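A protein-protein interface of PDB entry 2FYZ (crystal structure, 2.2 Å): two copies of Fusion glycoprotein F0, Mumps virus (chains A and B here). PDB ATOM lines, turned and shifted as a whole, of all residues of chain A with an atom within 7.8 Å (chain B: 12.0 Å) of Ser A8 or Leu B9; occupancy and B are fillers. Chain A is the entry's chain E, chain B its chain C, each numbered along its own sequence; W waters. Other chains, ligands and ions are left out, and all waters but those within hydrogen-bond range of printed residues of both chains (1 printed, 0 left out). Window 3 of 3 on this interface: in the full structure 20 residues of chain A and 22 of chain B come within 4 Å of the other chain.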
ATOM      1  N   LEU A   3     -19.708  18.067  13.977  1.00  0.00           N
ATOM      2  CA  LEU A   3     -19.375  16.708  13.588  1.00  0.00           C
ATOM      3  C   LEU A   3     -19.634  16.686  12.083  1.00  0.00           C
ATOM      4  O   LEU A   3     -18.874  16.107  11.311  1.00  0.00           O
ATOM      5  CB  LEU A   3     -20.293  15.712  14.335  1.00  0.00           C
ATOM      6  CG  LEU A   3     -19.978  14.215  14.298  1.00  0.00           C
ATOM      7  CD1 LEU A   3     -18.710  13.965  15.091  1.00  0.00           C
ATOM      8  CD2 LEU A   3     -21.127  13.399  14.883  1.00  0.00           C
ATOM      9  N   GLY A   4     -20.705  17.354  11.665  1.00  0.00           N
ATOM     10  CA  GLY A   4     -21.022  17.418  10.248  1.00  0.00           C
ATOM     11  C   GLY A   4     -19.871  18.033   9.470  1.00  0.00           C
ATOM     12  O   GLY A   4     -19.608  17.666   8.323  1.00  0.00           O
ATOM     13  N   SER A   5     -19.177  18.972  10.106  1.00  0.00           N
ATOM     14  CA  SER A   5     -18.032  19.623   9.486  1.00  0.00           C
ATOM     15  C   SER A   5     -16.912  18.595   9.373  1.00  0.00           C
ATOM     16  O   SER A   5     -16.246  18.484   8.342  1.00  0.00           O
ATOM     17  CB  SER A   5     -17.573  20.800  10.347  1.00  0.00           C
ATOM     18  OG  SER A   5     -16.342  21.314   9.877  1.00  0.00           O
ATOM     19  N   ALA A   6     -16.720  17.841  10.449  1.00  0.00           N
ATOM     20  CA  ALA A   6     -15.700  16.813  10.483  1.00  0.00           C
ATOM     21  C   ALA A   6     -16.009  15.745   9.434  1.00  0.00           C
ATOM     22  O   ALA A   6     -15.101  15.190   8.817  1.00  0.00           O
ATOM     23  CB  ALA A   6     -15.645  16.189  11.863  1.00  0.00           C
ATOM     24  N   VAL A   7     -17.297  15.469   9.240  1.00  0.00           N
ATOM     25  CA  VAL A   7     -17.754  14.466   8.281  1.00  0.00           C
ATOM     26  C   VAL A   7     -17.495  14.852   6.829  1.00  0.00           C
ATOM     27  O   VAL A   7     -17.083  14.014   6.026  1.00  0.00           O
ATOM     28  CB  VAL A   7     -19.265  14.185   8.458  1.00  0.00           C
ATOM     29  CG1 VAL A   7     -19.816  13.430   7.236  1.00  0.00           C
ATOM     30  CG2 VAL A   7     -19.482  13.368   9.727  1.00  0.00           C
ATOM     31  N   SER A   8     -17.742  16.115   6.489  1.00  0.00           N
ATOM     32  CA  SER A   8     -17.522  16.573   5.127  1.00  0.00           C
ATOM     33  C   SER A   8     -16.025  16.699   4.870  1.00  0.00           C
ATOM     34  O   SER A   8     -15.547  16.385   3.771  1.00  0.00           O
ATOM     35  CB  SER A   8     -18.220  17.916   4.888  1.00  0.00           C
ATOM     36  OG  SER A   8     -17.571  18.967   5.575  1.00  0.00           O
ATOM     37  N   LEU A   9     -15.288  17.150   5.884  1.00  0.00           N
ATOM     38  CA  LEU A   9     -13.841  17.297   5.757  1.00  0.00           C
ATOM     39  C   LEU A   9     -13.230  15.940   5.418  1.00  0.00           C
ATOM     40  O   LEU A   9     -12.345  15.842   4.574  1.00  0.00           O
ATOM     41  CB  LEU A   9     -13.242  17.841   7.059  1.00  0.00           C
ATOM     42  CG  LEU A   9     -11.712  17.859   7.240  1.00  0.00           C
ATOM     43  CD1 LEU A   9     -11.315  18.887   8.297  1.00  0.00           C
ATOM     44  CD2 LEU A   9     -11.218  16.485   7.650  1.00  0.00           C
ATOM     45  N   VAL A  10     -13.709  14.893   6.077  1.00  0.00           N
ATOM     46  CA  VAL A  10     -13.201  13.557   5.813  1.00  0.00           C
ATOM     47  C   VAL A  10     -13.642  13.078   4.426  1.00  0.00           C
ATOM     48  O   VAL A  10     -12.843  12.509   3.678  1.00  0.00           O
ATOM     49  CB  VAL A  10     -13.672  12.552   6.895  1.00  0.00           C
ATOM     50  CG1 VAL A  10     -13.311  11.122   6.491  1.00  0.00           C
ATOM     51  CG2 VAL A  10     -13.013  12.897   8.227  1.00  0.00           C
ATOM     52  N   GLN A  11     -14.906  13.317   4.080  1.00  0.00           N
ATOM     53  CA  GLN A  11     -15.406  12.899   2.777  1.00  0.00           C
ATOM     54  C   GLN A  11     -14.585  13.622   1.720  1.00  0.00           C
ATOM     55  O   GLN A  11     -14.211  13.033   0.704  1.00  0.00           O
ATOM     56  CB  GLN A  11     -16.887  13.252   2.620  1.00  0.00           C
ATOM     57  CG  GLN A  11     -17.549  12.656   1.371  1.00  0.00           C
ATOM     58  CD  GLN A  11     -17.808  11.154   1.488  1.00  0.00           C
ATOM     59  OE1 GLN A  11     -16.881  10.353   1.596  1.00  0.00           O
ATOM     60  NE2 GLN A  11     -19.080  10.772   1.465  1.00  0.00           N
ATOM     61  N   ALA A  12     -14.291  14.896   1.985  1.00  0.00           N
ATOM     62  CA  ALA A  12     -13.502  15.715   1.074  1.00  0.00           C
ATOM     63  C   ALA A  12     -12.120  15.111   0.865  1.00  0.00           C
ATOM     64  O   ALA A  12     -11.609  15.085  -0.251  1.00  0.00           O
ATOM     65  CB  ALA A  12     -13.371  17.128   1.623  1.00  0.00           C
ATOM     66  N   GLN A  13     -11.514  14.628   1.943  1.00  0.00           N
ATOM     67  CA  GLN A  13     -10.188  14.021   1.857  1.00  0.00           C
ATOM     68  C   GLN A  13     -10.253  12.679   1.143  1.00  0.00           C
ATOM     69  O   GLN A  13      -9.301  12.265   0.492  1.00  0.00           O
ATOM     70  CB  GLN A  13      -9.597  13.843   3.256  1.00  0.00           C
ATOM     71  CG  GLN A  13      -8.918  15.093   3.788  1.00  0.00           C
ATOM     72  CD  GLN A  13      -8.572  14.994   5.261  1.00  0.00           C
ATOM     73  OE1 GLN A  13      -8.234  13.921   5.766  1.00  0.00           O
ATOM     74  NE2 GLN A  13      -8.640  16.121   5.955  1.00  0.00           N
ATOM     75  N   THR A  14     -11.385  12.004   1.279  1.00  0.00           N
ATOM     76  CA  THR A  14     -11.587  10.720   0.632  1.00  0.00           C
ATOM     77  C   THR A  14     -11.729  10.948  -0.867  1.00  0.00           C
ATOM     78  O   THR A  14     -11.063  10.296  -1.668  1.00  0.00           O
ATOM     79  CB  THR A  14     -12.850  10.037   1.172  1.00  0.00           C
ATOM     80  OG1 THR A  14     -12.585   9.562   2.495  1.00  0.00           O
ATOM     81  CG2 THR A  14     -13.274   8.869   0.277  1.00  0.00           C
ATOM     82  N   ASN A  15     -12.591  11.888  -1.233  1.00  0.00           N
ATOM     83  CA  ASN A  15     -12.811  12.204  -2.631  1.00  0.00           C
ATOM     84  C   ASN A  15     -11.530  12.611  -3.346  1.00  0.00           C
ATOM     85  O   ASN A  15     -11.304  12.226  -4.491  1.00  0.00           O
ATOM     86  CB  ASN A  15     -13.864  13.305  -2.753  1.00  0.00           C
ATOM     87  CG  ASN A  15     -15.227  12.835  -2.305  1.00  0.00           C
ATOM     88  OD1 ASN A  15     -15.458  11.632  -2.180  1.00  0.00           O
ATOM     89  ND2 ASN A  15     -16.137  13.770  -2.068  1.00  0.00           N
ATOM     90  N   SER B   5     -20.200  24.797   7.198  1.00  0.00           N
ATOM     91  CA  SER B   5     -20.108  23.310   7.121  1.00  0.00           C
ATOM     92  C   SER B   5     -21.245  22.697   6.309  1.00  0.00           C
ATOM     93  O   SER B   5     -21.018  21.834   5.464  1.00  0.00           O
ATOM     94  CB  SER B   5     -20.108  22.712   8.531  1.00  0.00           C
ATOM     95  OG  SER B   5     -20.172  21.298   8.473  1.00  0.00           O
ATOM     96  N   ALA B   6     -22.467  23.148   6.573  1.00  0.00           N
ATOM     97  CA  ALA B   6     -23.643  22.637   5.878  1.00  0.00           C
ATOM     98  C   ALA B   6     -23.534  22.722   4.353  1.00  0.00           C
ATOM     99  O   ALA B   6     -24.258  22.039   3.631  1.00  0.00           O
ATOM    100  CB  ALA B   6     -24.893  23.373   6.367  1.00  0.00           C
ATOM    101  N   VAL B   7     -22.632  23.557   3.853  1.00  0.00           N
ATOM    102  CA  VAL B   7     -22.473  23.675   2.408  1.00  0.00           C
ATOM    103  C   VAL B   7     -21.461  22.654   1.914  1.00  0.00           C
ATOM    104  O   VAL B   7     -21.724  21.890   0.985  1.00  0.00           O
ATOM    105  CB  VAL B   7     -21.963  25.064   2.002  1.00  0.00           C
ATOM    106  CG1 VAL B   7     -22.000  25.183   0.494  1.00  0.00           C
ATOM    107  CG2 VAL B   7     -22.791  26.153   2.661  1.00  0.00           C
ATOM    108  N   SER B   8     -20.295  22.672   2.547  1.00  0.00           N
ATOM    109  CA  SER B   8     -19.213  21.758   2.225  1.00  0.00           C
ATOM    110  C   SER B   8     -19.709  20.317   2.350  1.00  0.00           C
ATOM    111  O   SER B   8     -19.157  19.401   1.733  1.00  0.00           O
ATOM    112  CB  SER B   8     -18.034  21.985   3.176  1.00  0.00           C
ATOM    113  OG  SER B   8     -18.457  21.926   4.531  1.00  0.00           O
ATOM    114  N   LEU B   9     -20.752  20.129   3.156  1.00  0.00           N
ATOM    115  CA  LEU B   9     -21.344  18.810   3.367  1.00  0.00           C
ATOM    116  C   LEU B   9     -21.970  18.338   2.062  1.00  0.00           C
ATOM    117  O   LEU B   9     -21.542  17.341   1.472  1.00  0.00           O
ATOM    118  CB  LEU B   9     -22.422  18.880   4.453  1.00  0.00           C
ATOM    119  CG  LEU B   9     -23.166  17.587   4.790  1.00  0.00           C
ATOM    120  CD1 LEU B   9     -22.200  16.579   5.399  1.00  0.00           C
ATOM    121  CD2 LEU B   9     -24.303  17.895   5.754  1.00  0.00           C
ATOM    122  N   VAL B  10     -22.988  19.073   1.624  1.00  0.00           N
ATOM    123  CA  VAL B  10     -23.697  18.779   0.388  1.00  0.00           C
ATOM    124  C   VAL B  10     -22.687  18.592  -0.739  1.00  0.00           C
ATOM    125  O   VAL B  10     -22.736  17.610  -1.477  1.00  0.00           O
ATOM    126  CB  VAL B  10     -24.650  19.940   0.028  1.00  0.00           C
ATOM    127  CG1 VAL B  10     -25.396  19.642  -1.261  1.00  0.00           C
ATOM    128  CG2 VAL B  10     -25.626  20.164   1.164  1.00  0.00           C
ATOM    129  N   GLN B  11     -21.767  19.542  -0.848  1.00  0.00           N
ATOM    130  CA  GLN B  11     -20.739  19.515  -1.873  1.00  0.00           C
ATOM    131  C   GLN B  11     -19.967  18.199  -1.844  1.00  0.00           C
ATOM    132  O   GLN B  11     -19.819  17.534  -2.872  1.00  0.00           O
ATOM    133  CB  GLN B  11     -19.780  20.689  -1.669  1.00  0.00           C
ATOM    134  CG  GLN B  11     -18.811  20.912  -2.817  1.00  0.00           C
ATOM    135  CD  GLN B  11     -19.517  21.223  -4.127  1.00  0.00           C
ATOM    136  OE1 GLN B  11     -20.720  21.486  -4.153  1.00  0.00           O
ATOM    137  NE2 GLN B  11     -18.766  21.205  -5.219  1.00  0.00           N
ATOM    138  N   ALA B  12     -19.478  17.832  -0.663  1.00  0.00           N
ATOM    139  CA  ALA B  12     -18.719  16.599  -0.487  1.00  0.00           C
ATOM    140  C   ALA B  12     -19.532  15.385  -0.919  1.00  0.00           C
ATOM    141  O   ALA B  12     -19.038  14.536  -1.653  1.00  0.00           O
ATOM    142  CB  ALA B  12     -18.287  16.448   0.969  1.00  0.00           C
ATOM    143  N   GLN B  13     -20.779  15.306  -0.468  1.00  0.00           N
ATOM    144  CA  GLN B  13     -21.639  14.185  -0.832  1.00  0.00           C
ATOM    145  C   GLN B  13     -21.827  14.170  -2.351  1.00  0.00           C
ATOM    146  O   GLN B  13     -21.692  13.131  -3.000  1.00  0.00           O
ATOM    147  CB  GLN B  13     -23.000  14.318  -0.145  1.00  0.00           C
ATOM    148  CG  GLN B  13     -22.917  14.685   1.331  1.00  0.00           C
ATOM    149  CD  GLN B  13     -24.283  14.948   1.958  1.00  0.00           C
ATOM    150  OE1 GLN B  13     -25.155  15.566   1.338  1.00  0.00           O
ATOM    151  NE2 GLN B  13     -24.468  14.491   3.196  1.00  0.00           N
ATOM    152  N   THR B  14     -22.134  15.335  -2.910  1.00  0.00           N
ATOM    153  CA  THR B  14     -22.338  15.463  -4.345  1.00  0.00           C
ATOM    154  C   THR B  14     -21.115  14.983  -5.127  1.00  0.00           C
ATOM    155  O   THR B  14     -21.238  14.184  -6.060  1.00  0.00           O
ATOM    156  CB  THR B  14     -22.656  16.926  -4.709  1.00  0.00           C
ATOM    157  OG1 THR B  14     -23.900  17.290  -4.102  1.00  0.00           O
ATOM    158  CG2 THR B  14     -22.754  17.109  -6.228  1.00  0.00           C
ATOM    159  N   ASN B  15     -19.936  15.461  -4.747  1.00  0.00           N
ATOM    160  CA  ASN B  15     -18.723  15.034  -5.426  1.00  0.00           C
ATOM    161  C   ASN B  15     -18.532  13.524  -5.272  1.00  0.00           C
ATOM    162  O   ASN B  15     -18.122  12.844  -6.212  1.00  0.00           O
ATOM    163  CB  ASN B  15     -17.513  15.796  -4.885  1.00  0.00           C
ATOM    164  CG  ASN B  15     -17.561  17.273  -5.234  1.00  0.00           C
ATOM    165  OD1 ASN B  15     -18.217  17.665  -6.199  1.00  0.00           O
ATOM    166  ND2 ASN B  15     -16.859  18.097  -4.464  1.00  0.00           N
ATOM    167  N   ALA B  16     -18.852  12.994  -4.097  1.00  0.00           N
ATOM    168  CA  ALA B  16     -18.726  11.559  -3.863  1.00  0.00           C
ATOM    169  C   ALA B  16     -19.577  10.790  -4.877  1.00  0.00           C
ATOM    170  O   ALA B  16     -19.115   9.814  -5.476  1.00  0.00           O
ATOM    171  CB  ALA B  16     -19.172  11.210  -2.440  1.00  0.00           C
ATOM    172  N   ARG B  17     -20.817  11.233  -5.068  1.00  0.00           N
ATOM    173  CA  ARG B  17     -21.712  10.573  -6.007  1.00  0.00           C
ATOM    174  C   ARG B  17     -21.244  10.758  -7.446  1.00  0.00           C
ATOM    175  O   ARG B  17     -21.416   9.868  -8.281  1.00  0.00           O
ATOM    176  CB  ARG B  17     -23.143  11.096  -5.854  1.00  0.00           C
ATOM    177  CG  ARG B  17     -23.892  10.517  -4.663  1.00  0.00           C
ATOM    178  CD  ARG B  17     -25.385  10.830  -4.737  1.00  0.00           C
ATOM    179  NE  ARG B  17     -25.649  12.264  -4.682  1.00  0.00           N
ATOM    180  CZ  ARG B  17     -25.474  13.014  -3.597  1.00  0.00           C
ATOM    181  NH1 ARG B  17     -25.038  12.465  -2.469  1.00  0.00           N
ATOM    182  NH2 ARG B  17     -25.728  14.316  -3.642  1.00  0.00           N
ATOM    183  N   ALA B  18     -20.660  11.915  -7.740  1.00  0.00           N
ATOM    184  CA  ALA B  18     -20.166  12.172  -9.086  1.00  0.00           C
ATOM    185  C   ALA B  18     -19.027  11.189  -9.371  1.00  0.00           C
ATOM    186  O   ALA B  18     -18.953  10.586 -10.442  1.00  0.00           O
ATOM    187  CB  ALA B  18     -19.670  13.609  -9.198  1.00  0.00           C
ATOM    188  N   ILE B  19     -18.148  11.020  -8.394  1.00  0.00           N
ATOM    189  CA  ILE B  19     -17.024  10.108  -8.531  1.00  0.00           C
ATOM    190  C   ILE B  19     -17.495   8.658  -8.681  1.00  0.00           C
ATOM    191  O   ILE B  19     -16.946   7.909  -9.479  1.00  0.00           O
ATOM    192  CB  ILE B  19     -16.082  10.242  -7.319  1.00  0.00           C
ATOM    193  CG1 ILE B  19     -15.463  11.647  -7.316  1.00  0.00           C
ATOM    194  CG2 ILE B  19     -15.002   9.165  -7.360  1.00  0.00           C
ATOM    195  CD1 ILE B  19     -14.753  12.009  -6.016  1.00  0.00           C
HETATM  196  O   HOH W   1     -15.185  16.977  -2.058  1.00  0.00           O
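Among the printed residues, merely in contact across the chains: Gly A4 with Ser B5, Ser A8 with Leu B9, Asn A15 with Ile B19, Asn A15 with Asn B15, Gln A11 with Ala B12, Ser A8 with Ala B12 and Gln A11 with Ala B16.
Of chain B, only Ser B5 (3.4 Å) comes within 4 Å of Gly A4.
Ser A5 touches one residue of chain B.
Val A7 touches none of the printed residues of chain B.
Of chain B, only Ser B8, Leu B9 and Ala B12 come within 4 Å of Ser A8.
No residue of chain B comes within 4 Å of Leu A9.
Gln A11 touches just these residues of chain B: Ala B12 (3.9 Å) and Ala B16 (3.9 Å).
No residue of chain B comes within 4 Å of Ala A12.
Printed residues of chain B within 4 Å of Asn A15: Ala B12 (3.0 Å), Asn B15 (3.7 Å), Ala B16 (3.5 Å) and Ile B19 (3.6 Å).
Printed residues of chain A within 4 Å of Leu B9: Ser A8 (3.6 Å).
Printed residues of chain A within 4 Å of Ala B12: Ser A8, Gln A11 and Asn A15.
Of the printed residues of chain A, Asn B15 touches Asn A15.
Of the printed residues of chain A, Ala B16 touches Gln A11 (3.9 Å) and Asn A15 (3.5 Å).
Of the printed residues of chain A, Ile B19 touches Asn A15.
The nearest residue of chain B that does not touch Ser A8 is Ser B5 (4.5 Å).
The nearest residue of chain A that does not touch Leu B9 is Gly A4 (4.1 Å).
Water W1 lies within hydrogen-bond range of the side-chain amide nitrogen of Asn B15 (3.1 Å) and the side-chain amide nitrogen of Asn A15 (3.3 Å).
The backbone carbonyl oxygen (O) of Ser B5 is in hydrogen-bond range of the side-chain hydroxyl (OG) of Ser B8, at 2.7 Å.
The backbone carbonyl oxygen (O) of Gln B11 sits close to the side-chain amide nitrogen (ND2) of Asn B15, 3.4 Å away.
O of Ser A5 sits at hydrogen-bond distance from OG of Ser A8 (3.1 Å).
O of Gln A11 lies close to OD1 of Asn A15 (3.4 Å).
N of Ser A5 lies close to OG of Ser B5, at 3.0 Å.
OG of Ser B8 is in hydrogen-bond range of OG of Ser A8 (3.3 Å).
ND2 of Asn A15 lies within hydrogen-bond range of O of Ala B12, at 3.0 Å.
The backbone NH (N) of Ala B16 sits close to the side-chain amide nitrogen (ND2) of Asn A15 (3.5 Å).
Ser B5 touches its own counterpart, Ser A5.
Ser B8 touches its own counterpart, Ser A8.
Gln A11 touches Ala B12, but with the chains exchanged Ala A12 does not touch Gln B11 (7.5 Å).
Asn A15 touches Ala B12, but with the chains exchanged Ala A12 does not touch Asn B15 (6.9 Å).
Positions printed for both chains: 5, 6, 7, 8, 9, 10, 11, 12, 13, 14 and 15.
Among the printed residues, no Asp or Glu carboxylate lies within 4 Å of a Lys or Arg side-chain nitrogen of the other chain.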
